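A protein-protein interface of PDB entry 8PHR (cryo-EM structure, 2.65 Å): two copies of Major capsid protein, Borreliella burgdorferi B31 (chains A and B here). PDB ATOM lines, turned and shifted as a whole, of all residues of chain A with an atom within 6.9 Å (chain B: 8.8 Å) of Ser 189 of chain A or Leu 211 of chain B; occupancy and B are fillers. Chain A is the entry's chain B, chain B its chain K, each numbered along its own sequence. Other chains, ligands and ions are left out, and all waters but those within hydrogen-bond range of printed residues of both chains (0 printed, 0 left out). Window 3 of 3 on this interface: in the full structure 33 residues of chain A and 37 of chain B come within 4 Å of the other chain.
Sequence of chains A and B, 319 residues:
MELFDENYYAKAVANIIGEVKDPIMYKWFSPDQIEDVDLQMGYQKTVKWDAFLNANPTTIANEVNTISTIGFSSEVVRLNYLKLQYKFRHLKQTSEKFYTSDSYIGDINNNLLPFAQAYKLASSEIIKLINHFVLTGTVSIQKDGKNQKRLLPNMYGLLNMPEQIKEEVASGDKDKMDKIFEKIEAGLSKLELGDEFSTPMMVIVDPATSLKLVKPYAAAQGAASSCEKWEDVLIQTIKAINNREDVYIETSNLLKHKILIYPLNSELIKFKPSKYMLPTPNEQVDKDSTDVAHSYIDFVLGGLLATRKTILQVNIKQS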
ATOM      1  N   GLU A 167     -10.765  12.772  29.552  1.00  0.00           N
ATOM      2  CA  GLU A 167     -10.868  11.667  30.492  1.00  0.00           C
ATOM      3  C   GLU A 167     -10.671  12.181  31.911  1.00  0.00           C
ATOM      4  O   GLU A 167      -9.949  13.157  32.143  1.00  0.00           O
ATOM      5  CB  GLU A 167      -9.839  10.573  30.182  1.00  0.00           C
ATOM      6  CG  GLU A 167      -9.812  10.149  28.722  1.00  0.00           C
ATOM      7  CD  GLU A 167     -10.887   9.131  28.391  1.00  0.00           C
ATOM      8  OE1 GLU A 167     -11.625   8.720  29.311  1.00  0.00           O
ATOM      9  OE2 GLU A 167     -10.996   8.747  27.208  1.00  0.00           O
ATOM     10  N   LYS A 183      -6.841   5.189  31.854  1.00  0.00           N
ATOM     11  CA  LYS A 183      -7.562   6.329  31.293  1.00  0.00           C
ATOM     12  C   LYS A 183      -6.830   6.905  30.084  1.00  0.00           C
ATOM     13  O   LYS A 183      -7.461   7.280  29.085  1.00  0.00           O
ATOM     14  CB  LYS A 183      -7.766   7.401  32.363  1.00  0.00           C
ATOM     15  CG  LYS A 183      -8.688   6.978  33.493  1.00  0.00           C
ATOM     16  CD  LYS A 183     -10.106   6.762  32.991  1.00  0.00           C
ATOM     17  CE  LYS A 183     -11.046   6.388  34.125  1.00  0.00           C
ATOM     18  NZ  LYS A 183     -12.463   6.318  33.671  1.00  0.00           N
ATOM     19  N   ILE A 184      -5.499   6.985  30.159  1.00  0.00           N
ATOM     20  CA  ILE A 184      -4.719   7.499  29.035  1.00  0.00           C
ATOM     21  C   ILE A 184      -4.871   6.595  27.817  1.00  0.00           C
ATOM     22  O   ILE A 184      -4.992   7.074  26.684  1.00  0.00           O
ATOM     23  CB  ILE A 184      -3.242   7.669  29.436  1.00  0.00           C
ATOM     24  CG1 ILE A 184      -3.102   8.731  30.528  1.00  0.00           C
ATOM     25  CG2 ILE A 184      -2.398   8.044  28.227  1.00  0.00           C
ATOM     26  CD1 ILE A 184      -1.701   8.856  31.083  1.00  0.00           C
ATOM     27  N   GLU A 185      -4.855   5.276  28.026  1.00  0.00           N
ATOM     28  CA  GLU A 185      -5.046   4.341  26.921  1.00  0.00           C
ATOM     29  C   GLU A 185      -6.433   4.483  26.310  1.00  0.00           C
ATOM     30  O   GLU A 185      -6.588   4.423  25.084  1.00  0.00           O
ATOM     31  CB  GLU A 185      -4.819   2.906  27.398  1.00  0.00           C
ATOM     32  CG  GLU A 185      -3.372   2.570  27.717  1.00  0.00           C
ATOM     33  CD  GLU A 185      -3.247   1.411  28.687  1.00  0.00           C
ATOM     34  OE1 GLU A 185      -4.291   0.877  29.114  1.00  0.00           O
ATOM     35  OE2 GLU A 185      -2.105   1.035  29.022  1.00  0.00           O
ATOM     36  N   ALA A 186      -7.456   4.661  27.149  1.00  0.00           N
ATOM     37  CA  ALA A 186      -8.804   4.868  26.627  1.00  0.00           C
ATOM     38  C   ALA A 186      -8.868   6.130  25.772  1.00  0.00           C
ATOM     39  O   ALA A 186      -9.440   6.125  24.674  1.00  0.00           O
ATOM     40  CB  ALA A 186      -9.807   4.942  27.778  1.00  0.00           C
ATOM     41  N   GLY A 187      -8.267   7.220  26.256  1.00  0.00           N
ATOM     42  CA  GLY A 187      -8.238   8.443  25.468  1.00  0.00           C
ATOM     43  C   GLY A 187      -7.469   8.288  24.169  1.00  0.00           C
ATOM     44  O   GLY A 187      -7.877   8.808  23.126  1.00  0.00           O
ATOM     45  N   LEU A 188      -6.342   7.575  24.215  1.00  0.00           N
ATOM     46  CA  LEU A 188      -5.545   7.351  23.016  1.00  0.00           C
ATOM     47  C   LEU A 188      -6.323   6.538  21.989  1.00  0.00           C
ATOM     48  O   LEU A 188      -6.241   6.803  20.784  1.00  0.00           O
ATOM     49  CB  LEU A 188      -4.240   6.643  23.380  1.00  0.00           C
ATOM     50  CG  LEU A 188      -3.134   7.478  24.030  1.00  0.00           C
ATOM     51  CD1 LEU A 188      -1.879   6.642  24.227  1.00  0.00           C
ATOM     52  CD2 LEU A 188      -2.826   8.723  23.223  1.00  0.00           C
ATOM     53  N   SER A 189      -7.081   5.541  22.449  1.00  0.00           N
ATOM     54  CA  SER A 189      -7.923   4.772  21.539  1.00  0.00           C
ATOM     55  C   SER A 189      -9.053   5.622  20.974  1.00  0.00           C
ATOM     56  O   SER A 189      -9.437   5.445  19.812  1.00  0.00           O
ATOM     57  CB  SER A 189      -8.488   3.543  22.252  1.00  0.00           C
ATOM     58  OG  SER A 189      -9.664   3.866  22.972  1.00  0.00           O
ATOM     59  N   LYS A 190      -9.592   6.547  21.771  1.00  0.00           N
ATOM     60  CA  LYS A 190     -10.632   7.441  21.276  1.00  0.00           C
ATOM     61  C   LYS A 190     -10.091   8.560  20.395  1.00  0.00           C
ATOM     62  O   LYS A 190     -10.886   9.259  19.758  1.00  0.00           O
ATOM     63  CB  LYS A 190     -11.414   8.046  22.444  1.00  0.00           C
ATOM     64  CG  LYS A 190     -12.146   7.026  23.298  1.00  0.00           C
ATOM     65  CD  LYS A 190     -12.682   7.662  24.569  1.00  0.00           C
ATOM     66  CE  LYS A 190     -13.227   6.615  25.526  1.00  0.00           C
ATOM     67  NZ  LYS A 190     -13.620   7.214  26.831  1.00  0.00           N
ATOM     68  N   LEU A 191      -8.774   8.752  20.347  1.00  0.00           N
ATOM     69  CA  LEU A 191      -8.200   9.737  19.436  1.00  0.00           C
ATOM     70  C   LEU A 191      -8.480   9.357  17.986  1.00  0.00           C
ATOM     71  O   LEU A 191      -8.514   8.179  17.622  1.00  0.00           O
ATOM     72  CB  LEU A 191      -6.691   9.862  19.657  1.00  0.00           C
ATOM     73  CG  LEU A 191      -6.196  10.836  20.727  1.00  0.00           C
ATOM     74  CD1 LEU A 191      -4.696  10.703  20.897  1.00  0.00           C
ATOM     75  CD2 LEU A 191      -6.552  12.263  20.353  1.00  0.00           C
ATOM     76  N   GLU A 192      -8.680  10.377  17.153  1.00  0.00           N
ATOM     77  CA  GLU A 192      -8.966  10.202  15.729  1.00  0.00           C
ATOM     78  C   GLU A 192      -8.046  11.131  14.944  1.00  0.00           C
ATOM     79  O   GLU A 192      -8.323  12.328  14.821  1.00  0.00           O
ATOM     80  CB  GLU A 192     -10.433  10.490  15.422  1.00  0.00           C
ATOM     81  CG  GLU A 192     -11.416   9.562  16.111  1.00  0.00           C
ATOM     82  CD  GLU A 192     -12.850   9.827  15.695  1.00  0.00           C
ATOM     83  OE1 GLU A 192     -13.069  10.745  14.876  1.00  0.00           O
ATOM     84  OE2 GLU A 192     -13.756   9.122  16.184  1.00  0.00           O
ATOM     85  N   GLN A 236       5.848   4.232  24.676  1.00  0.00           N
ATOM     86  CA  GLN A 236       5.515   3.090  23.829  1.00  0.00           C
ATOM     87  C   GLN A 236       4.030   3.067  23.486  1.00  0.00           C
ATOM     88  O   GLN A 236       3.648   2.751  22.352  1.00  0.00           O
ATOM     89  CB  GLN A 236       5.929   1.787  24.514  1.00  0.00           C
ATOM     90  CG  GLN A 236       7.431   1.636  24.696  1.00  0.00           C
ATOM     91  CD  GLN A 236       8.212   2.044  23.463  1.00  0.00           C
ATOM     92  OE1 GLN A 236       8.035   1.477  22.384  1.00  0.00           O
ATOM     93  NE2 GLN A 236       9.084   3.035  23.616  1.00  0.00           N
ATOM     94  N   THR A 237       3.172   3.405  24.452  1.00  0.00           N
ATOM     95  CA  THR A 237       1.736   3.425  24.189  1.00  0.00           C
ATOM     96  C   THR A 237       1.383   4.467  23.133  1.00  0.00           C
ATOM     97  O   THR A 237       0.546   4.216  22.257  1.00  0.00           O
ATOM     98  CB  THR A 237       0.968   3.689  25.484  1.00  0.00           C
ATOM     99  OG1 THR A 237       1.455   2.820  26.514  1.00  0.00           O
ATOM    100  CG2 THR A 237      -0.517   3.429  25.282  1.00  0.00           C
ATOM    101  N   ILE A 238       2.007   5.644  23.201  1.00  0.00           N
ATOM    102  CA  ILE A 238       1.750   6.681  22.203  1.00  0.00           C
ATOM    103  C   ILE A 238       2.336   6.286  20.851  1.00  0.00           C
ATOM    104  O   ILE A 238       1.774   6.607  19.793  1.00  0.00           O
ATOM    105  CB  ILE A 238       2.296   8.035  22.693  1.00  0.00           C
ATOM    106  CG1 ILE A 238       1.625   8.425  24.009  1.00  0.00           C
ATOM    107  CG2 ILE A 238       2.057   9.120  21.655  1.00  0.00           C
ATOM    108  CD1 ILE A 238       2.221   9.648  24.653  1.00  0.00           C
ATOM    109  N   ALA A 240       2.383   3.343  19.789  1.00  0.00           N
ATOM    110  CA  ALA A 240       1.434   2.378  19.248  1.00  0.00           C
ATOM    111  C   ALA A 240       0.352   3.032  18.396  1.00  0.00           C
ATOM    112  O   ALA A 240      -0.285   2.339  17.595  1.00  0.00           O
ATOM    113  CB  ALA A 240       0.783   1.584  20.380  1.00  0.00           C
ATOM    114  N   ILE A 241       0.128   4.336  18.544  1.00  0.00           N
ATOM    115  CA  ILE A 241      -0.893   5.026  17.766  1.00  0.00           C
ATOM    116  C   ILE A 241      -0.313   6.006  16.755  1.00  0.00           C
ATOM    117  O   ILE A 241      -0.986   6.303  15.756  1.00  0.00           O
ATOM    118  CB  ILE A 241      -1.908   5.750  18.676  1.00  0.00           C
ATOM    119  CG1 ILE A 241      -1.317   7.051  19.223  1.00  0.00           C
ATOM    120  CG2 ILE A 241      -2.344   4.850  19.817  1.00  0.00           C
ATOM    121  CD1 ILE A 241      -2.357   8.055  19.669  1.00  0.00           C
ATOM    122  N   LEU A 312      -6.175  15.134  23.569  1.00  0.00           N
ATOM    123  CA  LEU A 312      -6.547  14.319  24.716  1.00  0.00           C
ATOM    124  C   LEU A 312      -6.194  15.063  25.996  1.00  0.00           C
ATOM    125  O   LEU A 312      -5.056  15.519  26.164  1.00  0.00           O
ATOM    126  CB  LEU A 312      -5.846  12.959  24.678  1.00  0.00           C
ATOM    127  CG  LEU A 312      -6.018  12.081  25.918  1.00  0.00           C
ATOM    128  CD1 LEU A 312      -7.494  11.881  26.235  1.00  0.00           C
ATOM    129  CD2 LEU A 312      -5.327  10.742  25.725  1.00  0.00           C
ATOM    130  N   MET B 177      -5.219 -11.667  23.070  1.00  0.00           N
ATOM    131  CA  MET B 177      -3.972 -11.561  22.323  1.00  0.00           C
ATOM    132  C   MET B 177      -3.214 -12.881  22.321  1.00  0.00           C
ATOM    133  O   MET B 177      -2.486 -13.173  21.369  1.00  0.00           O
ATOM    134  CB  MET B 177      -3.108 -10.440  22.904  1.00  0.00           C
ATOM    135  CG  MET B 177      -1.760 -10.274  22.224  1.00  0.00           C
ATOM    136  SD  MET B 177      -1.915  -9.726  20.514  1.00  0.00           S
ATOM    137  CE  MET B 177      -0.553 -10.605  19.752  1.00  0.00           C
ATOM    138  N   VAL B 205      -0.585  -4.112  10.367  1.00  0.00           N
ATOM    139  CA  VAL B 205      -1.606  -4.348  11.379  1.00  0.00           C
ATOM    140  C   VAL B 205      -2.525  -3.136  11.468  1.00  0.00           C
ATOM    141  O   VAL B 205      -2.162  -2.018  11.099  1.00  0.00           O
ATOM    142  CB  VAL B 205      -0.994  -4.650  12.765  1.00  0.00           C
ATOM    143  CG1 VAL B 205      -0.254  -5.977  12.746  1.00  0.00           C
ATOM    144  CG2 VAL B 205      -0.068  -3.522  13.193  1.00  0.00           C
ATOM    145  N   ASP B 206      -3.732  -3.380  11.967  1.00  0.00           N
ATOM    146  CA  ASP B 206      -4.691  -2.322  12.232  1.00  0.00           C
ATOM    147  C   ASP B 206      -4.328  -1.584  13.519  1.00  0.00           C
ATOM    148  O   ASP B 206      -3.550  -2.087  14.335  1.00  0.00           O
ATOM    149  CB  ASP B 206      -6.099  -2.905  12.325  1.00  0.00           C
ATOM    150  CG  ASP B 206      -6.164  -4.132  13.209  1.00  0.00           C
ATOM    151  OD1 ASP B 206      -5.484  -5.129  12.893  1.00  0.00           O
ATOM    152  OD2 ASP B 206      -6.896  -4.099  14.222  1.00  0.00           O
ATOM    153  N   PRO B 207      -4.856  -0.368  13.709  1.00  0.00           N
ATOM    154  CA  PRO B 207      -4.559   0.364  14.954  1.00  0.00           C
ATOM    155  C   PRO B 207      -4.965  -0.381  16.215  1.00  0.00           C
ATOM    156  O   PRO B 207      -4.265  -0.289  17.232  1.00  0.00           O
ATOM    157  CB  PRO B 207      -5.349   1.668  14.781  1.00  0.00           C
ATOM    158  CG  PRO B 207      -5.432   1.854  13.305  1.00  0.00           C
ATOM    159  CD  PRO B 207      -5.585   0.470  12.741  1.00  0.00           C
ATOM    160  N   ALA B 208      -6.080  -1.113  16.184  1.00  0.00           N
ATOM    161  CA  ALA B 208      -6.477  -1.895  17.352  1.00  0.00           C
ATOM    162  C   ALA B 208      -5.450  -2.978  17.665  1.00  0.00           C
ATOM    163  O   ALA B 208      -5.094  -3.192  18.831  1.00  0.00           O
ATOM    164  CB  ALA B 208      -7.858  -2.510  17.130  1.00  0.00           C
ATOM    165  N   THR B 209      -4.959  -3.667  16.633  1.00  0.00           N
ATOM    166  CA  THR B 209      -3.923  -4.674  16.842  1.00  0.00           C
ATOM    167  C   THR B 209      -2.640  -4.038  17.359  1.00  0.00           C
ATOM    168  O   THR B 209      -1.963  -4.602  18.227  1.00  0.00           O
ATOM    169  CB  THR B 209      -3.664  -5.439  15.543  1.00  0.00           C
ATOM    170  OG1 THR B 209      -4.843  -6.166  15.173  1.00  0.00           O
ATOM    171  CG2 THR B 209      -2.512  -6.419  15.714  1.00  0.00           C
ATOM    172  N   SER B 210      -2.289  -2.858  16.841  1.00  0.00           N
ATOM    173  CA  SER B 210      -1.102  -2.163  17.327  1.00  0.00           C
ATOM    174  C   SER B 210      -1.243  -1.796  18.800  1.00  0.00           C
ATOM    175  O   SER B 210      -0.282  -1.905  19.570  1.00  0.00           O
ATOM    176  CB  SER B 210      -0.841  -0.915  16.484  1.00  0.00           C
ATOM    177  OG  SER B 210       0.412  -0.336  16.801  1.00  0.00           O
ATOM    178  N   LEU B 211      -2.435  -1.351  19.206  1.00  0.00           N
ATOM    179  CA  LEU B 211      -2.682  -1.069  20.617  1.00  0.00           C
ATOM    180  C   LEU B 211      -2.577  -2.332  21.462  1.00  0.00           C
ATOM    181  O   LEU B 211      -2.023  -2.303  22.568  1.00  0.00           O
ATOM    182  CB  LEU B 211      -4.055  -0.420  20.791  1.00  0.00           C
ATOM    183  CG  LEU B 211      -4.109   1.097  20.617  1.00  0.00           C
ATOM    184  CD1 LEU B 211      -5.484   1.631  20.985  1.00  0.00           C
ATOM    185  CD2 LEU B 211      -3.038   1.749  21.472  1.00  0.00           C
ATOM    186  N   LYS B 212      -3.112  -3.448  20.965  1.00  0.00           N
ATOM    187  CA  LYS B 212      -3.043  -4.696  21.722  1.00  0.00           C
ATOM    188  C   LYS B 212      -1.615  -5.224  21.821  1.00  0.00           C
ATOM    189  O   LYS B 212      -1.285  -5.931  22.780  1.00  0.00           O
ATOM    190  CB  LYS B 212      -3.954  -5.747  21.089  1.00  0.00           C
ATOM    191  CG  LYS B 212      -5.436  -5.410  21.150  1.00  0.00           C
ATOM    192  CD  LYS B 212      -6.283  -6.560  20.629  1.00  0.00           C
ATOM    193  CE  LYS B 212      -7.768  -6.257  20.756  1.00  0.00           C
ATOM    194  NZ  LYS B 212      -8.606  -7.346  20.181  1.00  0.00           N
ATOM    195  N   LEU B 213      -0.762  -4.899  20.845  1.00  0.00           N
ATOM    196  CA  LEU B 213       0.595  -5.441  20.832  1.00  0.00           C
ATOM    197  C   LEU B 213       1.424  -4.942  22.011  1.00  0.00           C
ATOM    198  O   LEU B 213       2.204  -5.705  22.591  1.00  0.00           O
ATOM    199  CB  LEU B 213       1.292  -5.092  19.516  1.00  0.00           C
ATOM    200  CG  LEU B 213       0.934  -5.904  18.272  1.00  0.00           C
ATOM    201  CD1 LEU B 213       1.928  -5.626  17.155  1.00  0.00           C
ATOM    202  CD2 LEU B 213       0.893  -7.388  18.593  1.00  0.00           C
ATOM    203  N   VAL B 214       1.272  -3.668  22.386  1.00  0.00           N
ATOM    204  CA  VAL B 214       2.151  -3.084  23.400  1.00  0.00           C
ATOM    205  C   VAL B 214       1.834  -3.548  24.810  1.00  0.00           C
ATOM    206  O   VAL B 214       2.589  -3.227  25.737  1.00  0.00           O
ATOM    207  CB  VAL B 214       2.109  -1.545  23.358  1.00  0.00           C
ATOM    208  CG1 VAL B 214       2.596  -1.045  22.009  1.00  0.00           C
ATOM    209  CG2 VAL B 214       0.707  -1.041  23.653  1.00  0.00           C
ATOM    210  N   LYS B 215       0.743  -4.285  25.006  1.00  0.00           N
ATOM    211  CA  LYS B 215       0.451  -4.833  26.319  1.00  0.00           C
ATOM    212  C   LYS B 215       1.524  -5.850  26.707  1.00  0.00           C
ATOM    213  O   LYS B 215       2.081  -6.537  25.844  1.00  0.00           O
ATOM    214  CB  LYS B 215      -0.929  -5.486  26.332  1.00  0.00           C
ATOM    215  CG  LYS B 215      -2.066  -4.537  25.991  1.00  0.00           C
ATOM    216  CD  LYS B 215      -3.376  -5.283  25.805  1.00  0.00           C
ATOM    217  CE  LYS B 215      -4.488  -4.340  25.373  1.00  0.00           C
ATOM    218  NZ  LYS B 215      -5.730  -5.073  24.999  1.00  0.00           N
ATOM    219  N   PRO B 216       1.847  -5.957  27.997  1.00  0.00           N
ATOM    220  CA  PRO B 216       2.908  -6.880  28.418  1.00  0.00           C
ATOM    221  C   PRO B 216       2.569  -8.324  28.078  1.00  0.00           C
ATOM    222  O   PRO B 216       1.410  -8.741  28.130  1.00  0.00           O
ATOM    223  CB  PRO B 216       2.990  -6.661  29.934  1.00  0.00           C
ATOM    224  CG  PRO B 216       2.365  -5.319  30.163  1.00  0.00           C
ATOM    225  CD  PRO B 216       1.287  -5.207  29.133  1.00  0.00           C
ATOM    226  N   TRP B 230       4.157  -8.302  23.717  1.00  0.00           N
ATOM    227  CA  TRP B 230       3.685  -9.118  22.603  1.00  0.00           C
ATOM    228  C   TRP B 230       4.368  -8.723  21.299  1.00  0.00           C
ATOM    229  O   TRP B 230       4.657  -9.580  20.459  1.00  0.00           O
ATOM    230  CB  TRP B 230       2.168  -8.997  22.470  1.00  0.00           C
ATOM    231  CG  TRP B 230       1.413  -9.759  23.514  1.00  0.00           C
ATOM    232  CD1 TRP B 230       0.701  -9.238  24.555  1.00  0.00           C
ATOM    233  CD2 TRP B 230       1.294 -11.182  23.619  1.00  0.00           C
ATOM    234  NE1 TRP B 230       0.147 -10.249  25.302  1.00  0.00           N
ATOM    235  CE2 TRP B 230       0.495 -11.453  24.748  1.00  0.00           C
ATOM    236  CE3 TRP B 230       1.786 -12.255  22.867  1.00  0.00           C
ATOM    237  CZ2 TRP B 230       0.177 -12.750  25.144  1.00  0.00           C
ATOM    238  CZ3 TRP B 230       1.469 -13.542  23.261  1.00  0.00           C
ATOM    239  CH2 TRP B 230       0.672 -13.779  24.390  1.00  0.00           C
ATOM    240  N   GLU B 231       4.628  -7.427  21.114  1.00  0.00           N
ATOM    241  CA  GLU B 231       5.324  -6.977  19.913  1.00  0.00           C
ATOM    242  C   GLU B 231       6.726  -7.569  19.837  1.00  0.00           C
ATOM    243  O   GLU B 231       7.151  -8.058  18.783  1.00  0.00           O
ATOM    244  CB  GLU B 231       5.379  -5.449  19.887  1.00  0.00           C
ATOM    245  CG  GLU B 231       6.207  -4.876  18.750  1.00  0.00           C
ATOM    246  CD  GLU B 231       6.062  -3.371  18.626  1.00  0.00           C
ATOM    247  OE1 GLU B 231       5.262  -2.783  19.384  1.00  0.00           O
ATOM    248  OE2 GLU B 231       6.748  -2.775  17.768  1.00  0.00           O
ATOM    249  N   THR B 251       1.416   0.282  10.641  1.00  0.00           N
ATOM    250  CA  THR B 251       0.007   0.430  10.973  1.00  0.00           C
ATOM    251  C   THR B 251      -0.701   1.134   9.825  1.00  0.00           C
ATOM    252  O   THR B 251      -0.232   2.171   9.345  1.00  0.00           O
ATOM    253  CB  THR B 251      -0.174   1.221  12.271  1.00  0.00           C
ATOM    254  OG1 THR B 251       0.754   0.749  13.255  1.00  0.00           O
ATOM    255  CG2 THR B 251      -1.591   1.059  12.799  1.00  0.00           C
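Of chain B, only Leu 211 comes within 4 Å of Ser 189 of chain A. Of the printed residues of chain A, Leu 211 of chain B touches Ser 189 (3.8 Å), Ala 240 (3.98 Å) and Ile 241 (3.6 Å). No residue of chain B comes within 4 Å of Gly 187 of chain A. Of the printed residues of chain A, Val 214 of chain B touches Gln 236 (3.95 Å) and Ala 240 (3.6 Å). Printed residues of chain B within 4 Å of Ile 241 of chain A: Leu 211. Of the printed residues of chain B, Ala 240 of chain A touches Ser 210, Leu 211 and Val 214. Printed residues of chain B within 4 Å of Gln 236 of chain A: Val 214 (3.95 Å). Ile 238 of chain A touches none of the printed residues of chain B. Lys 190 of chain A touches none of the printed residues of chain B. The nearest residue of chain B that does not touch Ser 189 of chain A is Pro 207 of chain B (7.5 Å). The nearest residue of chain A that does not touch Leu 211 of chain B is Thr 237 of chain A (4.4 Å). The nearest printed residue of chain A that does not touch Val 214 of chain B is Thr 237 of chain A (4.6 Å).
Hydrophobic or aromatic side chains of chain A within 4 Å of the printed part of chain B: Ala 240 and Ile 241. Of the 16 printed residues of chain B, 3 touch a printed residue of chain A. Printed residues of chain B that touch a printed residue of chain A: Ser 210, Leu 211 and Val 214. Among the printed residues, no Asp or Glu carboxylate lies within 4 Å of a Lys or Arg side-chain nitrogen of the other chain.
No position is printed for both chains. Of the 6 pairs that touch across the chains among the printed residues, none has its exchanged pair printed and touching as well.
OG of Ser 210 of chain B lies within hydrogen-bond range of O of Ala 240 of chain A (2.9 Å).
The backbone carbonyl oxygen (O) of Ala 186 of chain A is in hydrogen-bond range of the side-chain hydroxyl (OG) of Ser 189 of chain A, 2.8 Å away.
Ser 189 of chain A touches Leu 211 of chain B. CG1 of Val 214 of chain B touches O of Gln 236 of chain A (3.95 Å). Ala 240 of chain A touches Leu 211 of chain B (CB to CD2, 3.98 Å). Ala 240 of chain A touches Val 214 of chain B. Ile 241 of chain A touches Leu 211 of chain B.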
